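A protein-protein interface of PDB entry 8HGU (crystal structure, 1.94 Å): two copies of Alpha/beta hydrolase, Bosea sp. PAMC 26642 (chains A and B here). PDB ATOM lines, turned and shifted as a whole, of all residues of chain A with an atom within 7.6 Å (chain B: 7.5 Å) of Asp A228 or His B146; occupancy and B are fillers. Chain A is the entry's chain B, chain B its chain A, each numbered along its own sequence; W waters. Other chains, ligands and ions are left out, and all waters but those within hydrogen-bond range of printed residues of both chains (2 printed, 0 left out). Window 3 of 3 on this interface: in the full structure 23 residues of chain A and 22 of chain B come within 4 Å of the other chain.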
ATOM      1  N   GLY A 140      -3.901   4.126 -24.746  1.00  0.00           N
ATOM      2  CA  GLY A 140      -4.363   4.983 -23.638  1.00  0.00           C
ATOM      3  C   GLY A 140      -4.520   6.425 -24.085  1.00  0.00           C
ATOM      4  O   GLY A 140      -5.211   6.660 -25.065  1.00  0.00           O
ATOM      5  N   GLY A 141      -3.805   7.342 -23.461  1.00  0.00           N
ATOM      6  CA  GLY A 141      -3.944   8.787 -23.736  1.00  0.00           C
ATOM      7  C   GLY A 141      -3.427   9.175 -25.109  1.00  0.00           C
ATOM      8  O   GLY A 141      -3.831  10.247 -25.628  1.00  0.00           O
ATOM      9  N   VAL A 144      -5.593  10.624 -27.924  1.00  0.00           N
ATOM     10  CA  VAL A 144      -6.143  12.014 -27.977  1.00  0.00           C
ATOM     11  C   VAL A 144      -5.073  13.090 -27.783  1.00  0.00           C
ATOM     12  O   VAL A 144      -5.432  14.267 -27.985  1.00  0.00           O
ATOM     13  CB  VAL A 144      -7.300  12.210 -26.990  1.00  0.00           C
ATOM     14  CG1 VAL A 144      -8.496  11.374 -27.397  1.00  0.00           C
ATOM     15  CG2 VAL A 144      -6.903  11.931 -25.547  1.00  0.00           C
ATOM     16  N   LEU A 222     -14.661   0.693 -23.399  1.00  0.00           N
ATOM     17  CA  LEU A 222     -13.251   0.218 -23.263  1.00  0.00           C
ATOM     18  C   LEU A 222     -12.313   1.342 -23.718  1.00  0.00           C
ATOM     19  O   LEU A 222     -11.326   1.596 -23.063  1.00  0.00           O
ATOM     20  CB  LEU A 222     -13.007  -1.041 -24.099  1.00  0.00           C
ATOM     21  CG  LEU A 222     -13.619  -2.354 -23.590  1.00  0.00           C
ATOM     22  CD1 LEU A 222     -13.410  -3.465 -24.622  1.00  0.00           C
ATOM     23  CD2 LEU A 222     -13.042  -2.781 -22.237  1.00  0.00           C
ATOM     24  N   ARG A 223     -12.630   1.979 -24.828  1.00  0.00           N
ATOM     25  CA  ARG A 223     -11.817   3.084 -25.397  1.00  0.00           C
ATOM     26  C   ARG A 223     -11.759   4.228 -24.362  1.00  0.00           C
ATOM     27  O   ARG A 223     -10.663   4.703 -24.091  1.00  0.00           O
ATOM     28  CB  ARG A 223     -12.390   3.489 -26.765  1.00  0.00           C
ATOM     29  CG  ARG A 223     -11.722   4.674 -27.456  1.00  0.00           C
ATOM     30  CD  ARG A 223     -10.263   4.508 -27.807  1.00  0.00           C
ATOM     31  NE  ARG A 223      -9.921   3.150 -28.197  1.00  0.00           N
ATOM     32  CZ  ARG A 223     -10.033   2.645 -29.429  1.00  0.00           C
ATOM     33  NH1 ARG A 223     -10.461   3.382 -30.447  1.00  0.00           N
ATOM     34  NH2 ARG A 223      -9.724   1.376 -29.630  1.00  0.00           N
ATOM     35  N   LEU A 224     -12.881   4.627 -23.770  1.00  0.00           N
ATOM     36  CA  LEU A 224     -12.892   5.755 -22.807  1.00  0.00           C
ATOM     37  C   LEU A 224     -12.084   5.395 -21.538  1.00  0.00           C
ATOM     38  O   LEU A 224     -11.341   6.265 -21.036  1.00  0.00           O
ATOM     39  CB  LEU A 224     -14.332   6.059 -22.407  1.00  0.00           C
ATOM     40  CG  LEU A 224     -15.276   6.616 -23.462  1.00  0.00           C
ATOM     41  CD1 LEU A 224     -16.548   7.073 -22.767  1.00  0.00           C
ATOM     42  CD2 LEU A 224     -14.654   7.735 -24.240  1.00  0.00           C
ATOM     43  N   ALA A 225     -12.133   4.142 -21.088  1.00  0.00           N
ATOM     44  CA  ALA A 225     -11.378   3.683 -19.905  1.00  0.00           C
ATOM     45  C   ALA A 225      -9.882   3.784 -20.227  1.00  0.00           C
ATOM     46  O   ALA A 225      -9.137   4.367 -19.386  1.00  0.00           O
ATOM     47  CB  ALA A 225     -11.792   2.293 -19.485  1.00  0.00           C
ATOM     48  N   ALA A 226      -9.465   3.301 -21.404  1.00  0.00           N
ATOM     49  CA  ALA A 226      -8.058   3.346 -21.882  1.00  0.00           C
ATOM     50  C   ALA A 226      -7.557   4.800 -21.940  1.00  0.00           C
ATOM     51  O   ALA A 226      -6.481   5.096 -21.332  1.00  0.00           O
ATOM     52  CB  ALA A 226      -7.911   2.656 -23.209  1.00  0.00           C
ATOM     53  N   ILE A 227      -8.331   5.712 -22.546  1.00  0.00           N
ATOM     54  CA  ILE A 227      -7.937   7.144 -22.698  1.00  0.00           C
ATOM     55  C   ILE A 227      -7.634   7.772 -21.336  1.00  0.00           C
ATOM     56  O   ILE A 227      -6.703   8.557 -21.274  1.00  0.00           O
ATOM     57  CB  ILE A 227      -9.009   7.938 -23.453  1.00  0.00           C
ATOM     58  CG1 ILE A 227      -9.017   7.518 -24.918  1.00  0.00           C
ATOM     59  CG2 ILE A 227      -8.788   9.426 -23.286  1.00  0.00           C
ATOM     60  CD1 ILE A 227     -10.212   7.961 -25.687  1.00  0.00           C
ATOM     61  N   ASP A 228      -8.386   7.454 -20.282  1.00  0.00           N
ATOM     62  CA  ASP A 228      -8.199   8.026 -18.922  1.00  0.00           C
ATOM     63  C   ASP A 228      -7.180   7.208 -18.137  1.00  0.00           C
ATOM     64  O   ASP A 228      -7.030   7.472 -16.969  1.00  0.00           O
ATOM     65  CB  ASP A 228      -9.534   8.118 -18.180  1.00  0.00           C
ATOM     66  CG  ASP A 228     -10.481   9.178 -18.763  1.00  0.00           C
ATOM     67  OD1 ASP A 228     -10.061   9.960 -19.665  1.00  0.00           O
ATOM     68  OD2 ASP A 228     -11.641   9.210 -18.344  1.00  0.00           O
ATOM     69  N   GLY A 229      -6.497   6.248 -18.754  1.00  0.00           N
ATOM     70  CA  GLY A 229      -5.395   5.527 -18.104  1.00  0.00           C
ATOM     71  C   GLY A 229      -5.877   4.480 -17.117  1.00  0.00           C
ATOM     72  O   GLY A 229      -5.067   4.103 -16.269  1.00  0.00           O
ATOM     73  N   HIS A 230      -7.115   3.978 -17.254  1.00  0.00           N
ATOM     74  CA  HIS A 230      -7.717   2.930 -16.382  1.00  0.00           C
ATOM     75  C   HIS A 230      -8.269   1.795 -17.236  1.00  0.00           C
ATOM     76  O   HIS A 230      -9.438   1.463 -17.104  1.00  0.00           O
ATOM     77  CB  HIS A 230      -8.857   3.511 -15.508  1.00  0.00           C
ATOM     78  CG  HIS A 230      -8.517   4.754 -14.749  1.00  0.00           C
ATOM     79  ND1 HIS A 230      -7.599   4.766 -13.689  1.00  0.00           N
ATOM     80  CD2 HIS A 230      -8.979   6.026 -14.862  1.00  0.00           C
ATOM     81  CE1 HIS A 230      -7.496   5.991 -13.202  1.00  0.00           C
ATOM     82  NE2 HIS A 230      -8.334   6.787 -13.909  1.00  0.00           N
ATOM     83  N   PRO A 231      -7.497   1.169 -18.154  1.00  0.00           N
ATOM     84  CA  PRO A 231      -8.018   0.036 -18.928  1.00  0.00           C
ATOM     85  C   PRO A 231      -8.174  -1.163 -17.989  1.00  0.00           C
ATOM     86  O   PRO A 231      -7.485  -1.179 -17.004  1.00  0.00           O
ATOM     87  CB  PRO A 231      -6.915  -0.219 -19.968  1.00  0.00           C
ATOM     88  CG  PRO A 231      -5.652   0.299 -19.320  1.00  0.00           C
ATOM     89  CD  PRO A 231      -6.088   1.448 -18.444  1.00  0.00           C
ATOM     90  N   GLY B 141      -6.943  19.453 -20.753  1.00  0.00           N
ATOM     91  CA  GLY B 141      -7.145  18.010 -20.952  1.00  0.00           C
ATOM     92  C   GLY B 141      -8.583  17.587 -20.699  1.00  0.00           C
ATOM     93  O   GLY B 141      -8.978  16.519 -21.210  1.00  0.00           O
ATOM     94  N   ALA B 142      -9.382  18.415 -20.008  1.00  0.00           N
ATOM     95  CA  ALA B 142     -10.812  18.128 -19.794  1.00  0.00           C
ATOM     96  C   ALA B 142     -11.584  18.147 -21.134  1.00  0.00           C
ATOM     97  O   ALA B 142     -12.654  17.525 -21.169  1.00  0.00           O
ATOM     98  CB  ALA B 142     -11.406  19.030 -18.731  1.00  0.00           C
ATOM     99  N   TRP B 143     -11.049  18.734 -22.214  1.00  0.00           N
ATOM    100  CA  TRP B 143     -11.678  18.641 -23.570  1.00  0.00           C
ATOM    101  C   TRP B 143     -11.727  17.180 -24.035  1.00  0.00           C
ATOM    102  O   TRP B 143     -12.606  16.872 -24.817  1.00  0.00           O
ATOM    103  CB  TRP B 143     -10.955  19.492 -24.607  1.00  0.00           C
ATOM    104  CG  TRP B 143     -11.262  20.954 -24.557  1.00  0.00           C
ATOM    105  CD1 TRP B 143     -10.422  21.973 -24.193  1.00  0.00           C
ATOM    106  CD2 TRP B 143     -12.515  21.566 -24.891  1.00  0.00           C
ATOM    107  NE1 TRP B 143     -11.067  23.181 -24.296  1.00  0.00           N
ATOM    108  CE2 TRP B 143     -12.360  22.963 -24.707  1.00  0.00           C
ATOM    109  CE3 TRP B 143     -13.749  21.073 -25.324  1.00  0.00           C
ATOM    110  CZ2 TRP B 143     -13.390  23.870 -24.982  1.00  0.00           C
ATOM    111  CZ3 TRP B 143     -14.761  21.968 -25.583  1.00  0.00           C
ATOM    112  CH2 TRP B 143     -14.583  23.344 -25.416  1.00  0.00           C
ATOM    113  N   VAL B 144     -10.817  16.312 -23.597  1.00  0.00           N
ATOM    114  CA  VAL B 144     -10.681  14.946 -24.191  1.00  0.00           C
ATOM    115  C   VAL B 144     -10.732  13.824 -23.148  1.00  0.00           C
ATOM    116  O   VAL B 144     -10.635  12.657 -23.590  1.00  0.00           O
ATOM    117  CB  VAL B 144      -9.428  14.803 -25.061  1.00  0.00           C
ATOM    118  CG1 VAL B 144      -9.514  15.668 -26.298  1.00  0.00           C
ATOM    119  CG2 VAL B 144      -8.131  15.041 -24.324  1.00  0.00           C
ATOM    120  N   HIS B 145     -10.859  14.119 -21.851  1.00  0.00           N
ATOM    121  CA  HIS B 145     -10.865  13.092 -20.789  1.00  0.00           C
ATOM    122  C   HIS B 145     -12.275  12.940 -20.206  1.00  0.00           C
ATOM    123  O   HIS B 145     -13.177  13.745 -20.532  1.00  0.00           O
ATOM    124  CB  HIS B 145      -9.747  13.401 -19.768  1.00  0.00           C
ATOM    125  CG  HIS B 145      -8.375  13.092 -20.286  1.00  0.00           C
ATOM    126  ND1 HIS B 145      -7.929  11.787 -20.475  1.00  0.00           N
ATOM    127  CD2 HIS B 145      -7.357  13.886 -20.677  1.00  0.00           C
ATOM    128  CE1 HIS B 145      -6.695  11.801 -20.960  1.00  0.00           C
ATOM    129  NE2 HIS B 145      -6.319  13.070 -21.100  1.00  0.00           N
ATOM    130  N   HIS B 146     -12.481  11.902 -19.398  1.00  0.00           N
ATOM    131  CA  HIS B 146     -13.738  11.669 -18.647  1.00  0.00           C
ATOM    132  C   HIS B 146     -14.897  11.551 -19.636  1.00  0.00           C
ATOM    133  O   HIS B 146     -16.010  12.014 -19.343  1.00  0.00           O
ATOM    134  CB  HIS B 146     -13.889  12.762 -17.576  1.00  0.00           C
ATOM    135  CG  HIS B 146     -12.777  12.725 -16.578  1.00  0.00           C
ATOM    136  ND1 HIS B 146     -11.794  13.706 -16.506  1.00  0.00           N
ATOM    137  CD2 HIS B 146     -12.451  11.793 -15.655  1.00  0.00           C
ATOM    138  CE1 HIS B 146     -10.919  13.383 -15.574  1.00  0.00           C
ATOM    139  NE2 HIS B 146     -11.307  12.217 -15.028  1.00  0.00           N
ATOM    140  N   GLY B 147     -14.646  10.924 -20.772  1.00  0.00           N
ATOM    141  CA  GLY B 147     -15.688  10.712 -21.778  1.00  0.00           C
ATOM    142  C   GLY B 147     -15.866  11.867 -22.731  1.00  0.00           C
ATOM    143  O   GLY B 147     -16.602  11.669 -23.748  1.00  0.00           O
ATOM    144  N   HIS B 148     -15.190  13.004 -22.542  1.00  0.00           N
ATOM    145  CA  HIS B 148     -15.537  14.211 -23.335  1.00  0.00           C
ATOM    146  C   HIS B 148     -15.100  14.074 -24.786  1.00  0.00           C
ATOM    147  O   HIS B 148     -15.631  14.831 -25.643  1.00  0.00           O
ATOM    148  CB  HIS B 148     -14.984  15.477 -22.708  1.00  0.00           C
ATOM    149  CG  HIS B 148     -15.860  16.644 -22.995  1.00  0.00           C
ATOM    150  ND1 HIS B 148     -17.125  16.735 -22.497  1.00  0.00           N
ATOM    151  CD2 HIS B 148     -15.637  17.808 -23.640  1.00  0.00           C
ATOM    152  CE1 HIS B 148     -17.689  17.867 -22.928  1.00  0.00           C
ATOM    153  NE2 HIS B 148     -16.823  18.523 -23.600  1.00  0.00           N
ATOM    154  N   VAL B 149     -14.232  13.098 -25.091  1.00  0.00           N
ATOM    155  CA  VAL B 149     -13.749  12.940 -26.480  1.00  0.00           C
ATOM    156  C   VAL B 149     -14.953  12.650 -27.374  1.00  0.00           C
ATOM    157  O   VAL B 149     -14.910  13.054 -28.570  1.00  0.00           O
ATOM    158  CB  VAL B 149     -12.663  11.844 -26.608  1.00  0.00           C
ATOM    159  CG1 VAL B 149     -13.249  10.457 -26.384  1.00  0.00           C
ATOM    160  CG2 VAL B 149     -11.995  11.911 -27.969  1.00  0.00           C
ATOM    161  N   ASN B 150     -16.022  12.073 -26.825  1.00  0.00           N
ATOM    162  CA  ASN B 150     -17.206  11.688 -27.625  1.00  0.00           C
ATOM    163  C   ASN B 150     -17.970  12.964 -28.021  1.00  0.00           C
ATOM    164  O   ASN B 150     -18.667  12.924 -29.052  1.00  0.00           O
ATOM    165  CB  ASN B 150     -18.165  10.747 -26.911  1.00  0.00           C
ATOM    166  CG  ASN B 150     -17.616   9.344 -26.720  1.00  0.00           C
ATOM    167  OD1 ASN B 150     -17.851   8.659 -25.705  1.00  0.00           O
ATOM    168  ND2 ASN B 150     -16.896   8.919 -27.726  1.00  0.00           N
ATOM    169  N   LYS B 253     -19.017  21.789 -20.273  1.00  0.00           N
ATOM    170  CA  LYS B 253     -19.523  21.183 -19.021  1.00  0.00           C
ATOM    171  C   LYS B 253     -19.630  22.272 -17.948  1.00  0.00           C
ATOM    172  O   LYS B 253     -18.718  23.091 -17.845  1.00  0.00           O
ATOM    173  CB  LYS B 253     -18.629  20.015 -18.591  1.00  0.00           C
ATOM    174  CG  LYS B 253     -18.550  18.858 -19.589  1.00  0.00           C
ATOM    175  CD  LYS B 253     -17.786  17.654 -19.041  1.00  0.00           C
ATOM    176  CE  LYS B 253     -18.633  16.827 -18.099  1.00  0.00           C
ATOM    177  NZ  LYS B 253     -17.836  16.395 -16.927  1.00  0.00           N
HETATM  178  O   HOH W   1     -12.124   9.045 -21.390  1.00  0.00           O
HETATM  179  O   HOH W   2     -13.985   8.046 -19.142  1.00  0.00           O
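Water W2 lies within hydrogen-bond range of OD2 of Asp A228 (2.7 Å) and N of Gly B147 (3.4 Å).
Water W1 lies within hydrogen-bond range of the side-chain carboxylate of Asp A228 (2.8 Å), the backbone carbonyl oxygen of Leu A224 (2.9 Å) and the backbone NH of Gly B147 (3.2 Å).
Val A144 touches its own counterpart, Val B144.
2 positions are printed for both chains.
Of the 10 pairs that touch across the chains among the printed residues, 1 has its exchanged pair printed and touching as well.
Among the printed residues, pairs that only touch across the chains: Val A144 with Val B144, Val A144 with Val B149, Leu A224 with Gly B147, Leu A224 with Val B149, Leu A224 with Asn B150, Ile A227 with Val B144, Ile A227 with His B145 and Ile A227 with Val B149.
O of Asp A228 lies close to NE2 of His A230, 3.4 Å away.
Of the printed residues of chain B, Val A144 touches Val B144 (3.6 Å) and Val B149 (3.6 Å).
Asp A228 touches two residues of chain B.
Of the printed residues of chain A, Val B144 touches Val A144 (3.6 Å) and Ile A227 (3.7 Å).
Of the printed residues of chain A, His B145 touches Ile A227 (3.3 Å) and Asp A228 (2.9 Å).
His B146 touches just one residue of chain A: Asp A228.
Of the printed residues of chain A, Gly B147 touches Leu A224 (3.9 Å).
Of the printed residues of chain A, Val B149 touches Val A144, Leu A224 and Ile A227.
The nearest printed residue of chain A that does not touch Val B144 is Asp A228 (4.8 Å).
A ring nitrogen (ND1) of His B145 is in hydrogen-bond range of the side-chain carboxylate of Asp A228 (2.9 Å).
The backbone NH of His B146 is in hydrogen-bond range of the side-chain carboxylate of Asp A228, 3.0 Å away.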
